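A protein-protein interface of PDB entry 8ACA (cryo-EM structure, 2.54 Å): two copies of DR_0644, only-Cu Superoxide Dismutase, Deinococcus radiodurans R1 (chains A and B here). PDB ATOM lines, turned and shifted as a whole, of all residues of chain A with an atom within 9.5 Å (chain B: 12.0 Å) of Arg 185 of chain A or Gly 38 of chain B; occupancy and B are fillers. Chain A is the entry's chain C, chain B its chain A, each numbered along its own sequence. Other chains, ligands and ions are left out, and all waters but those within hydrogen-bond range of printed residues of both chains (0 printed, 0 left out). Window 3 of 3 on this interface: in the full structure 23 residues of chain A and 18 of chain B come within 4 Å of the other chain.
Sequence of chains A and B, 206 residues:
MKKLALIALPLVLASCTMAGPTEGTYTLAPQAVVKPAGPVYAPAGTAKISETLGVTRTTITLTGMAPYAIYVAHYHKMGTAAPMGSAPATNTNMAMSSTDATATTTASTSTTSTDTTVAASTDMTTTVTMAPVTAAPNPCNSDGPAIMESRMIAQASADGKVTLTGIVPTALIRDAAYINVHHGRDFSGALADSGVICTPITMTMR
Among the printed residues, pairs that only touch across the chains: Arg 185 of chain A with Gly 38 of chain B (3.8 Å), Asp 186 of chain A with Tyr 68 of chain B (3.6 Å), Leu 191 of chain A with Ala 37 of chain B (3.3 Å), Ala 192 of chain A with Pro 36 of chain B (3.4 Å), Asp 193 of chain A with Val 34 of chain B (3.6 Å), Asp 193 of chain A with Lys 35 of chain B (3.7 Å) and Ser 194 of chain A with Val 34 of chain B (3.8 Å).
The backbone carbonyl oxygen of Ala 192 of chain A lies within hydrogen-bond range of the backbone NH of Ala 37 of chain B (2.7 Å). The backbone carbonyl oxygen (O) of Lys 35 of chain B lies within hydrogen-bond range of the backbone NH (N) of Ser 194 of chain A (2.9 Å).
No residue of chain B comes within 4 Å of Ile 70 of chain A. No residue of chain B comes within 4 Å of Gly 184 of chain A. Arg 185 of chain A touches just one residue of chain B: Gly 38 (3.8 Å). Asp 186 of chain A touches just one residue of chain B: Tyr 68 (3.6 Å). Leu 191 of chain A touches just one residue of chain B: Ala 37 (3.3 Å). Ala 192 of chain A touches just these residues of chain B: Pro 36 and Ala 37. Printed residues of chain B within 4 Å of Asp 193 of chain A: Val 34 (3.6 Å) and Lys 35 (3.7 Å). Printed residues of chain A within 4 Å of Lys 35 of chain B: Asp 193 (3.7 Å) and Ser 194 (2.9 Å). Ala 37 of chain B touches just these residues of chain A: Leu 191 and Ala 192. Pro 39 of chain B touches none of the printed residues of chain A. Thr 63 of chain B touches none of the printed residues of chain A. Gly 64 of chain B touches none of the printed residues of chain A. The nearest residue of chain A that does not touch Gly 38 of chain B is Leu 191 of chain A (4.8 Å). The nearest printed residue of chain A that does not touch Val 34 of chain B is His 183 of chain A (5.8 Å).
The backbone carbonyl oxygen (O) of Asp 193 of chain A lies close to a ring nitrogen (ND1) of His 182 of chain A, 3.4 Å away. A ring nitrogen (ND1) of His 183 of chain A lies within hydrogen-bond range of the side-chain carboxylate of Asp 193 of chain A (2.9 Å). The backbone NH (N) of Ala 192 of chain A is in hydrogen-bond range of the backbone carbonyl oxygen (O) of His 183 of chain A (2.9 Å). The backbone carbonyl oxygen (O) of Leu 191 of chain A lies within hydrogen-bond range of the guanidinium group (NH1) of Arg 185 of chain A.
Of the 20 printed residues of chain A, 6 touch a printed residue of chain B. Of the 21 printed residues of chain B, 6 touch a printed residue of chain A.
No position is printed for both chains. Of the 9 pairs that touch across the chains among the printed residues, none has its exchanged pair printed and touching as well.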
ATOM      1  N   ALA A  69       3.808   9.849   5.712  1.00  0.00           N
ATOM      2  CA  ALA A  69       3.751   8.526   6.367  1.00  0.00           C
ATOM      3  C   ALA A  69       3.837   7.394   5.347  1.00  0.00           C
ATOM      4  O   ALA A  69       3.289   7.543   4.256  1.00  0.00           O
ATOM      5  CB  ALA A  69       2.518   8.427   7.216  1.00  0.00           C
ATOM      6  N   ILE A  70       4.525   6.314   5.704  1.00  0.00           N
ATOM      7  CA  ILE A  70       4.620   5.115   4.823  1.00  0.00           C
ATOM      8  C   ILE A  70       3.285   4.382   4.926  1.00  0.00           C
ATOM      9  O   ILE A  70       2.779   4.263   6.048  1.00  0.00           O
ATOM     10  CB  ILE A  70       5.763   4.222   5.331  1.00  0.00           C
ATOM     11  CG1 ILE A  70       7.123   4.904   5.173  1.00  0.00           C
ATOM     12  CG2 ILE A  70       5.740   2.855   4.674  1.00  0.00           C
ATOM     13  CD1 ILE A  70       8.246   4.195   5.885  1.00  0.00           C
ATOM     14  N   TYR A  71       2.726   3.914   3.804  1.00  0.00           N
ATOM     15  CA  TYR A  71       1.382   3.278   3.837  1.00  0.00           C
ATOM     16  C   TYR A  71       1.409   1.916   3.136  1.00  0.00           C
ATOM     17  O   TYR A  71       0.975   1.843   1.979  1.00  0.00           O
ATOM     18  CB  TYR A  71       0.347   4.194   3.177  1.00  0.00           C
ATOM     19  CG  TYR A  71      -0.314   5.180   4.107  1.00  0.00           C
ATOM     20  CD1 TYR A  71      -1.384   4.806   4.901  1.00  0.00           C
ATOM     21  CD2 TYR A  71       0.126   6.490   4.189  1.00  0.00           C
ATOM     22  CE1 TYR A  71      -1.998   5.705   5.756  1.00  0.00           C
ATOM     23  CE2 TYR A  71      -0.479   7.404   5.037  1.00  0.00           C
ATOM     24  CZ  TYR A  71      -1.546   7.010   5.823  1.00  0.00           C
ATOM     25  OH  TYR A  71      -2.150   7.900   6.662  1.00  0.00           O
ATOM     26  N   VAL A  72       1.868   0.868   3.826  1.00  0.00           N
ATOM     27  CA  VAL A  72       1.901  -0.500   3.242  1.00  0.00           C
ATOM     28  C   VAL A  72       0.478  -0.912   2.897  1.00  0.00           C
ATOM     29  O   VAL A  72      -0.372  -0.906   3.797  1.00  0.00           O
ATOM     30  CB  VAL A  72       2.504  -1.496   4.241  1.00  0.00           C
ATOM     31  CG1 VAL A  72       2.642  -2.886   3.642  1.00  0.00           C
ATOM     32  CG2 VAL A  72       3.840  -1.003   4.763  1.00  0.00           C
ATOM     33  N   ILE A 153       4.217  -0.622  -1.254  1.00  0.00           N
ATOM     34  CA  ILE A 153       4.690   0.359  -0.233  1.00  0.00           C
ATOM     35  C   ILE A 153       4.825   1.737  -0.886  1.00  0.00           C
ATOM     36  O   ILE A 153       5.142   1.757  -2.085  1.00  0.00           O
ATOM     37  CB  ILE A 153       6.016  -0.109   0.395  1.00  0.00           C
ATOM     38  CG1 ILE A 153       5.836  -1.390   1.211  1.00  0.00           C
ATOM     39  CG2 ILE A 153       6.644   0.993   1.229  1.00  0.00           C
ATOM     40  CD1 ILE A 153       7.136  -2.021   1.620  1.00  0.00           C
ATOM     41  N   ALA A 154       4.570   2.825  -0.147  1.00  0.00           N
ATOM     42  CA  ALA A 154       4.771   4.208  -0.653  1.00  0.00           C
ATOM     43  C   ALA A 154       4.730   5.186   0.516  1.00  0.00           C
ATOM     44  O   ALA A 154       4.236   4.793   1.574  1.00  0.00           O
ATOM     45  CB  ALA A 154       3.739   4.595  -1.668  1.00  0.00           C
ATOM     46  N   GLN A 155       5.222   6.408   0.319  1.00  0.00           N
ATOM     47  CA  GLN A 155       5.152   7.434   1.389  1.00  0.00           C
ATOM     48  C   GLN A 155       4.281   8.572   0.885  1.00  0.00           C
ATOM     49  O   GLN A 155       4.084   8.648  -0.330  1.00  0.00           O
ATOM     50  CB  GLN A 155       6.533   7.973   1.748  1.00  0.00           C
ATOM     51  CG  GLN A 155       6.668   8.340   3.217  1.00  0.00           C
ATOM     52  CD  GLN A 155       8.002   8.955   3.550  1.00  0.00           C
ATOM     53  OE1 GLN A 155       8.845   9.159   2.682  1.00  0.00           O
ATOM     54  NE2 GLN A 155       8.201   9.259   4.821  1.00  0.00           N
ATOM     55  N   HIS A 182      -2.617  -0.196   5.320  1.00  0.00           N
ATOM     56  CA  HIS A 182      -2.173  -0.088   6.736  1.00  0.00           C
ATOM     57  C   HIS A 182      -1.139   1.032   6.851  1.00  0.00           C
ATOM     58  O   HIS A 182      -0.909   1.724   5.842  1.00  0.00           O
ATOM     59  CB  HIS A 182      -1.534  -1.399   7.209  1.00  0.00           C
ATOM     60  CG  HIS A 182      -2.375  -2.616   7.016  1.00  0.00           C
ATOM     61  ND1 HIS A 182      -3.040  -3.223   8.061  1.00  0.00           N
ATOM     62  CD2 HIS A 182      -2.634  -3.360   5.919  1.00  0.00           C
ATOM     63  CE1 HIS A 182      -3.691  -4.278   7.613  1.00  0.00           C
ATOM     64  NE2 HIS A 182      -3.459  -4.381   6.301  1.00  0.00           N
ATOM     65  N   HIS A 183      -0.542   1.214   8.023  1.00  0.00           N
ATOM     66  CA  HIS A 183       0.552   2.210   8.164  1.00  0.00           C
ATOM     67  C   HIS A 183       1.874   1.446   8.193  1.00  0.00           C
ATOM     68  O   HIS A 183       1.874   0.302   8.683  1.00  0.00           O
ATOM     69  CB  HIS A 183       0.372   3.048   9.431  1.00  0.00           C
ATOM     70  CG  HIS A 183      -0.369   4.335   9.230  1.00  0.00           C
ATOM     71  ND1 HIS A 183      -1.575   4.621   9.818  1.00  0.00           N
ATOM     72  CD2 HIS A 183      -0.029   5.417   8.476  1.00  0.00           C
ATOM     73  CE1 HIS A 183      -1.965   5.835   9.444  1.00  0.00           C
ATOM     74  NE2 HIS A 183      -1.020   6.349   8.615  1.00  0.00           N
ATOM     75  N   GLY A 184       2.946   2.049   7.685  1.00  0.00           N
ATOM     76  CA  GLY A 184       4.248   1.362   7.611  1.00  0.00           C
ATOM     77  C   GLY A 184       5.225   1.885   8.646  1.00  0.00           C
ATOM     78  O   GLY A 184       5.534   3.093   8.606  1.00  0.00           O
ATOM     79  N   ARG A 185       5.693   1.013   9.542  1.00  0.00           N
ATOM     80  CA  ARG A 185       6.693   1.423  10.562  1.00  0.00           C
ATOM     81  C   ARG A 185       8.025   1.672   9.851  1.00  0.00           C
ATOM     82  O   ARG A 185       8.802   2.518  10.338  1.00  0.00           O
ATOM     83  CB  ARG A 185       6.843   0.327  11.621  1.00  0.00           C
ATOM     84  CG  ARG A 185       5.623   0.153  12.515  1.00  0.00           C
ATOM     85  CD  ARG A 185       5.934  -0.704  13.726  1.00  0.00           C
ATOM     86  NE  ARG A 185       6.311  -2.059  13.350  1.00  0.00           N
ATOM     87  CZ  ARG A 185       5.451  -3.049  13.134  1.00  0.00           C
ATOM     88  NH1 ARG A 185       4.153  -2.835  13.257  1.00  0.00           N
ATOM     89  NH2 ARG A 185       5.893  -4.247  12.794  1.00  0.00           N
ATOM     90  N   ASP A 186       8.270   0.968   8.739  1.00  0.00           N
ATOM     91  CA  ASP A 186       9.546   1.115   7.987  1.00  0.00           C
ATOM     92  C   ASP A 186       9.272   1.006   6.483  1.00  0.00           C
ATOM     93  O   ASP A 186       8.195   0.491   6.123  1.00  0.00           O
ATOM     94  CB  ASP A 186      10.573   0.071   8.429  1.00  0.00           C
ATOM     95  CG  ASP A 186      11.431   0.524   9.596  1.00  0.00           C
ATOM     96  OD1 ASP A 186      12.308   1.384   9.379  1.00  0.00           O
ATOM     97  OD2 ASP A 186      11.212   0.018  10.714  1.00  0.00           O
ATOM     98  N   PHE A 187      10.199   1.486   5.646  1.00  0.00           N
ATOM     99  CA  PHE A 187      10.046   1.380   4.177  1.00  0.00           C
ATOM    100  C   PHE A 187      10.191  -0.085   3.795  1.00  0.00           C
ATOM    101  O   PHE A 187       9.888  -0.424   2.647  1.00  0.00           O
ATOM    102  CB  PHE A 187      11.113   2.212   3.465  1.00  0.00           C
ATOM    103  CG  PHE A 187      11.029   3.695   3.707  1.00  0.00           C
ATOM    104  CD1 PHE A 187      10.163   4.483   2.969  1.00  0.00           C
ATOM    105  CD2 PHE A 187      11.822   4.302   4.665  1.00  0.00           C
ATOM    106  CE1 PHE A 187      10.087   5.849   3.190  1.00  0.00           C
ATOM    107  CE2 PHE A 187      11.747   5.667   4.883  1.00  0.00           C
ATOM    108  CZ  PHE A 187      10.881   6.437   4.146  1.00  0.00           C
ATOM    109  N   SER A 188      10.635  -0.923   4.734  1.00  0.00           N
ATOM    110  CA  SER A 188      10.744  -2.383   4.466  1.00  0.00           C
ATOM    111  C   SER A 188       9.374  -3.020   4.669  1.00  0.00           C
ATOM    112  O   SER A 188       9.247  -4.231   4.425  1.00  0.00           O
ATOM    113  CB  SER A 188      11.774  -3.031   5.341  1.00  0.00           C
ATOM    114  OG  SER A 188      11.395  -2.945   6.705  1.00  0.00           O
ATOM    115  N   GLY A 189       8.389  -2.242   5.129  1.00  0.00           N
ATOM    116  CA  GLY A 189       7.029  -2.774   5.353  1.00  0.00           C
ATOM    117  C   GLY A 189       6.554  -2.551   6.776  1.00  0.00           C
ATOM    118  O   GLY A 189       6.517  -1.374   7.185  1.00  0.00           O
ATOM    119  N   ALA A 190       6.171  -3.621   7.487  1.00  0.00           N
ATOM    120  CA  ALA A 190       5.705  -3.542   8.899  1.00  0.00           C
ATOM    121  C   ALA A 190       4.303  -2.921   8.998  1.00  0.00           C
ATOM    122  O   ALA A 190       4.021  -1.944   8.280  1.00  0.00           O
ATOM    123  CB  ALA A 190       6.720  -2.840   9.772  1.00  0.00           C
ATOM    124  N   LEU A 191       3.450  -3.470   9.867  1.00  0.00           N
ATOM    125  CA  LEU A 191       2.049  -2.977   9.970  1.00  0.00           C
ATOM    126  C   LEU A 191       1.877  -2.165  11.257  1.00  0.00           C
ATOM    127  O   LEU A 191       1.299  -2.714  12.216  1.00  0.00           O
ATOM    128  CB  LEU A 191       1.100  -4.179   9.973  1.00  0.00           C
ATOM    129  CG  LEU A 191       0.991  -4.937   8.652  1.00  0.00           C
ATOM    130  CD1 LEU A 191      -0.281  -5.770   8.620  1.00  0.00           C
ATOM    131  CD2 LEU A 191       1.036  -3.978   7.473  1.00  0.00           C
ATOM    132  N   ALA A 192       2.368  -0.918  11.278  1.00  0.00           N
ATOM    133  CA  ALA A 192       2.180  -0.033  12.455  1.00  0.00           C
ATOM    134  C   ALA A 192       0.709  -0.072  12.847  1.00  0.00           C
ATOM    135  O   ALA A 192       0.400  -0.450  13.995  1.00  0.00           O
ATOM    136  CB  ALA A 192       2.571   1.378  12.094  1.00  0.00           C
ATOM    137  N   ASP A 193      -0.155   0.327  11.915  1.00  0.00           N
ATOM    138  CA  ASP A 193      -1.619   0.300  12.166  1.00  0.00           C
ATOM    139  C   ASP A 193      -2.180  -0.959  11.504  1.00  0.00           C
ATOM    140  O   ASP A 193      -1.494  -1.521  10.628  1.00  0.00           O
ATOM    141  CB  ASP A 193      -2.308   1.556  11.627  1.00  0.00           C
ATOM    142  CG  ASP A 193      -2.057   2.795  12.468  1.00  0.00           C
ATOM    143  OD1 ASP A 193      -1.140   2.757  13.311  1.00  0.00           O
ATOM    144  OD2 ASP A 193      -2.781   3.791  12.270  1.00  0.00           O
ATOM    145  N   SER A 194      -3.377  -1.380  11.913  1.00  0.00           N
ATOM    146  CA  SER A 194      -3.985  -2.617  11.354  1.00  0.00           C
ATOM    147  C   SER A 194      -5.231  -2.283  10.527  1.00  0.00           C
ATOM    148  O   SER A 194      -6.297  -2.857  10.823  1.00  0.00           O
ATOM    149  CB  SER A 194      -4.302  -3.601  12.449  1.00  0.00           C
ATOM    150  OG  SER A 194      -3.112  -4.054  13.077  1.00  0.00           O
ATOM    151  N   VAL B  34      -9.305   1.170  13.943  1.00  0.00           N
ATOM    152  CA  VAL B  34      -7.940   0.767  13.490  1.00  0.00           C
ATOM    153  C   VAL B  34      -7.103   0.489  14.746  1.00  0.00           C
ATOM    154  O   VAL B  34      -7.131   1.334  15.664  1.00  0.00           O
ATOM    155  CB  VAL B  34      -7.307   1.836  12.577  1.00  0.00           C
ATOM    156  CG1 VAL B  34      -7.405   3.233  13.170  1.00  0.00           C
ATOM    157  CG2 VAL B  34      -5.873   1.502  12.204  1.00  0.00           C
ATOM    158  N   LYS B  35      -6.412  -0.655  14.803  1.00  0.00           N
ATOM    159  CA  LYS B  35      -5.680  -1.016  16.049  1.00  0.00           C
ATOM    160  C   LYS B  35      -4.168  -0.970  15.807  1.00  0.00           C
ATOM    161  O   LYS B  35      -3.715  -1.558  14.811  1.00  0.00           O
ATOM    162  CB  LYS B  35      -6.097  -2.408  16.536  1.00  0.00           C
ATOM    163  CG  LYS B  35      -7.535  -2.533  17.020  1.00  0.00           C
ATOM    164  CD  LYS B  35      -7.899  -3.933  17.465  1.00  0.00           C
ATOM    165  CE  LYS B  35      -9.324  -4.044  17.967  1.00  0.00           C
ATOM    166  NZ  LYS B  35      -9.657  -5.429  18.373  1.00  0.00           N
ATOM    167  N   PRO B  36      -3.367  -0.306  16.668  1.00  0.00           N
ATOM    168  CA  PRO B  36      -1.905  -0.314  16.526  1.00  0.00           C
ATOM    169  C   PRO B  36      -1.301  -1.696  16.824  1.00  0.00           C
ATOM    170  O   PRO B  36      -1.838  -2.400  17.661  1.00  0.00           O
ATOM    171  CB  PRO B  36      -1.432   0.719  17.560  1.00  0.00           C
ATOM    172  CG  PRO B  36      -2.547   0.766  18.584  1.00  0.00           C
ATOM    173  CD  PRO B  36      -3.819   0.501  17.803  1.00  0.00           C
ATOM    174  N   ALA B  37      -0.211  -2.051  16.136  1.00  0.00           N
ATOM    175  CA  ALA B  37       0.445  -3.364  16.350  1.00  0.00           C
ATOM    176  C   ALA B  37       1.873  -3.159  16.874  1.00  0.00           C
ATOM    177  O   ALA B  37       2.107  -2.134  17.547  1.00  0.00           O
ATOM    178  CB  ALA B  37       0.432  -4.164  15.071  1.00  0.00           C
ATOM    179  N   GLY B  38       2.784  -4.094  16.580  1.00  0.00           N
ATOM    180  CA  GLY B  38       4.168  -4.007  17.096  1.00  0.00           C
ATOM    181  C   GLY B  38       4.308  -4.214  18.586  1.00  0.00           C
ATOM    182  O   GLY B  38       3.445  -4.865  19.190  1.00  0.00           O
ATOM    183  N   PRO B  39       5.395  -3.716  19.203  1.00  0.00           N
ATOM    184  CA  PRO B  39       5.629  -3.874  20.641  1.00  0.00           C
ATOM    185  C   PRO B  39       4.545  -3.332  21.582  1.00  0.00           C
ATOM    186  O   PRO B  39       3.865  -2.398  21.225  1.00  0.00           O
ATOM    187  CB  PRO B  39       6.903  -3.051  20.863  1.00  0.00           C
ATOM    188  CG  PRO B  39       7.618  -3.169  19.547  1.00  0.00           C
ATOM    189  CD  PRO B  39       6.496  -3.018  18.545  1.00  0.00           C
ATOM    190  N   VAL B  40       4.394  -3.960  22.750  1.00  0.00           N
ATOM    191  CA  VAL B  40       3.416  -3.466  23.764  1.00  0.00           C
ATOM    192  C   VAL B  40       4.227  -2.884  24.927  1.00  0.00           C
ATOM    193  O   VAL B  40       5.145  -3.580  25.406  1.00  0.00           O
ATOM    194  CB  VAL B  40       2.458  -4.585  24.220  1.00  0.00           C
ATOM    195  CG1 VAL B  40       3.196  -5.719  24.918  1.00  0.00           C
ATOM    196  CG2 VAL B  40       1.323  -4.062  25.089  1.00  0.00           C
ATOM    197  N   TYR B  41       3.935  -1.642  25.322  1.00  0.00           N
ATOM    198  CA  TYR B  41       4.710  -0.988  26.406  1.00  0.00           C
ATOM    199  C   TYR B  41       4.383  -1.660  27.743  1.00  0.00           C
ATOM    200  O   TYR B  41       3.515  -1.142  28.474  1.00  0.00           O
ATOM    201  CB  TYR B  41       4.444   0.519  26.446  1.00  0.00           C
ATOM    202  CG  TYR B  41       5.436   1.297  27.271  1.00  0.00           C
ATOM    203  CD1 TYR B  41       6.800   1.112  27.111  1.00  0.00           C
ATOM    204  CD2 TYR B  41       5.016   2.213  28.221  1.00  0.00           C
ATOM    205  CE1 TYR B  41       7.719   1.819  27.866  1.00  0.00           C
ATOM    206  CE2 TYR B  41       5.922   2.929  28.984  1.00  0.00           C
ATOM    207  CZ  TYR B  41       7.278   2.732  28.807  1.00  0.00           C
ATOM    208  OH  TYR B  41       8.177   3.432  29.557  1.00  0.00           O
ATOM    209  N   ALA B  42       5.047  -2.780  28.043  1.00  0.00           N
ATOM    210  CA  ALA B  42       4.845  -3.460  29.337  1.00  0.00           C
ATOM    211  C   ALA B  42       6.181  -3.466  30.090  1.00  0.00           C
ATOM    212  O   ALA B  42       6.789  -4.540  30.094  1.00  0.00           O
ATOM    213  CB  ALA B  42       4.377  -4.852  29.094  1.00  0.00           C
ATOM    214  N   THR B  63      12.783  -5.836  29.320  1.00  0.00           N
ATOM    215  CA  THR B  63      12.070  -6.266  28.100  1.00  0.00           C
ATOM    216  C   THR B  63      10.681  -5.639  28.110  1.00  0.00           C
ATOM    217  O   THR B  63      10.166  -5.391  29.198  1.00  0.00           O
ATOM    218  CB  THR B  63      12.023  -7.794  27.988  1.00  0.00           C
ATOM    219  OG1 THR B  63      11.565  -8.313  29.237  1.00  0.00           O
ATOM    220  CG2 THR B  63      13.364  -8.401  27.642  1.00  0.00           C
ATOM    221  N   GLY B  64      10.119  -5.397  26.935  1.00  0.00           N
ATOM    222  CA  GLY B  64       8.762  -4.842  26.844  1.00  0.00           C
ATOM    223  C   GLY B  64       8.790  -3.343  26.955  1.00  0.00           C
ATOM    224  O   GLY B  64       7.775  -2.770  27.346  1.00  0.00           O
ATOM    225  N   MET B  65       9.902  -2.719  26.564  1.00  0.00           N
ATOM    226  CA  MET B  65      10.088  -1.260  26.756  1.00  0.00           C
ATOM    227  C   MET B  65       9.617  -0.534  25.495  1.00  0.00           C
ATOM    228  O   MET B  65       8.856  -1.138  24.728  1.00  0.00           O
ATOM    229  CB  MET B  65      11.561  -0.953  27.026  1.00  0.00           C
ATOM    230  CG  MET B  65      12.045  -1.454  28.360  1.00  0.00           C
ATOM    231  SD  MET B  65      10.961  -0.890  29.680  1.00  0.00           S
ATOM    232  CE  MET B  65      12.155  -0.186  30.811  1.00  0.00           C
ATOM    233  N   ALA B  66      10.051   0.715  25.302  1.00  0.00           N
ATOM    234  CA  ALA B  66       9.634   1.533  24.132  1.00  0.00           C
ATOM    235  C   ALA B  66      10.529   1.198  22.951  1.00  0.00           C
ATOM    236  O   ALA B  66      11.743   1.251  23.133  1.00  0.00           O
ATOM    237  CB  ALA B  66       9.667   3.003  24.452  1.00  0.00           C
ATOM    238  N   PRO B  67       9.998   0.904  21.748  1.00  0.00           N
ATOM    239  CA  PRO B  67      10.815   0.412  20.636  1.00  0.00           C
ATOM    240  C   PRO B  67      12.235   0.953  20.439  1.00  0.00           C
ATOM    241  O   PRO B  67      13.085   0.143  20.527  1.00  0.00           O
ATOM    242  CB  PRO B  67       9.916   0.444  19.404  1.00  0.00           C
ATOM    243  CG  PRO B  67       8.518   0.412  19.978  1.00  0.00           C
ATOM    244  CD  PRO B  67       8.594   1.020  21.366  1.00  0.00           C
ATOM    245  N   TYR B  68      12.474   2.237  20.176  1.00  0.00           N
ATOM    246  CA  TYR B  68      13.891   2.668  20.011  1.00  0.00           C
ATOM    247  C   TYR B  68      14.204   3.829  20.939  1.00  0.00           C
ATOM    248  O   TYR B  68      14.663   4.847  20.437  1.00  0.00           O
ATOM    249  CB  TYR B  68      14.229   3.147  18.606  1.00  0.00           C
ATOM    250  CG  TYR B  68      13.769   2.336  17.423  1.00  0.00           C
ATOM    251  CD1 TYR B  68      14.683   1.655  16.641  1.00  0.00           C
ATOM    252  CD2 TYR B  68      12.445   2.328  17.022  1.00  0.00           C
ATOM    253  CE1 TYR B  68      14.287   0.934  15.529  1.00  0.00           C
ATOM    254  CE2 TYR B  68      12.028   1.603  15.921  1.00  0.00           C
ATOM    255  CZ  TYR B  68      12.955   0.910  15.167  1.00  0.00           C
ATOM    256  OH  TYR B  68      12.556   0.206  14.071  1.00  0.00           O
ATOM    257  N   ALA B 156      16.774   0.693  23.108  1.00  0.00           N
ATOM    258  CA  ALA B 156      15.937  -0.518  23.292  1.00  0.00           C
ATOM    259  C   ALA B 156      15.686  -1.289  21.990  1.00  0.00           C
ATOM    260  O   ALA B 156      14.573  -1.827  21.866  1.00  0.00           O
ATOM    261  CB  ALA B 156      14.640  -0.134  23.959  1.00  0.00           C
ATOM    262  N   SER B 157      16.675  -1.387  21.091  1.00  0.00           N
ATOM    263  CA  SER B 157      16.520  -2.196  19.850  1.00  0.00           C
ATOM    264  C   SER B 157      15.296  -1.730  19.049  1.00  0.00           C
ATOM    265  O   SER B 157      15.258  -0.537  18.702  1.00  0.00           O
ATOM    266  CB  SER B 157      16.457  -3.674  20.153  1.00  0.00           C
ATOM    267  OG  SER B 157      17.466  -4.042  21.081  1.00  0.00           O
ATOM    268  N   ALA B 158      14.323  -2.613  18.785  1.00  0.00           N
ATOM    269  CA  ALA B 158      13.148  -2.247  17.951  1.00  0.00           C
ATOM    270  C   ALA B 158      11.880  -2.921  18.488  1.00  0.00           C
ATOM    271  O   ALA B 158      10.799  -2.661  17.927  1.00  0.00           O
ATOM    272  CB  ALA B 158      13.403  -2.644  16.518  1.00  0.00           C
ATOM    273  N   ASP B 159      12.065  -3.775  19.496  1.00  0.00           N
ATOM    274  CA  ASP B 159      10.924  -4.465  20.142  1.00  0.00           C
ATOM    275  C   ASP B 159      10.896  -4.002  21.599  1.00  0.00           C
ATOM    276  O   ASP B 159       9.947  -4.385  22.313  1.00  0.00           O
ATOM    277  CB  ASP B 159      11.077  -5.984  20.041  1.00  0.00           C
ATOM    278  CG  ASP B 159       9.919  -6.742  20.669  1.00  0.00           C
ATOM    279  OD1 ASP B 159       8.791  -6.622  20.151  1.00  0.00           O
ATOM    280  OD2 ASP B 159      10.156  -7.442  21.672  1.00  0.00           O
ATOM    281  N   GLY B 160      11.891  -3.211  22.027  1.00  0.00           N
ATOM    282  CA  GLY B 160      11.788  -2.718  23.403  1.00  0.00           C
ATOM    283  C   GLY B 160      12.664  -3.535  24.316  1.00  0.00           C
ATOM    284  O   GLY B 160      12.296  -3.720  25.472  1.00  0.00           O
ATOM    285  N   LYS B 161      13.789  -4.012  23.800  1.00  0.00           N
ATOM    286  CA  LYS B 161      14.728  -4.824  24.599  1.00  0.00           C
ATOM    287  C   LYS B 161      15.978  -3.992  24.851  1.00  0.00           C
ATOM    288  O   LYS B 161      16.743  -3.813  23.910  1.00  0.00           O
ATOM    289  CB  LYS B 161      15.032  -6.130  23.865  1.00  0.00           C
ATOM    290  CG  LYS B 161      13.822  -7.022  23.642  1.00  0.00           C
ATOM    291  CD  LYS B 161      14.162  -8.335  22.981  1.00  0.00           C
ATOM    292  CE  LYS B 161      14.919  -9.280  23.890  1.00  0.00           C
ATOM    293  NZ  LYS B 161      14.069  -9.761  25.002  1.00  0.00           N
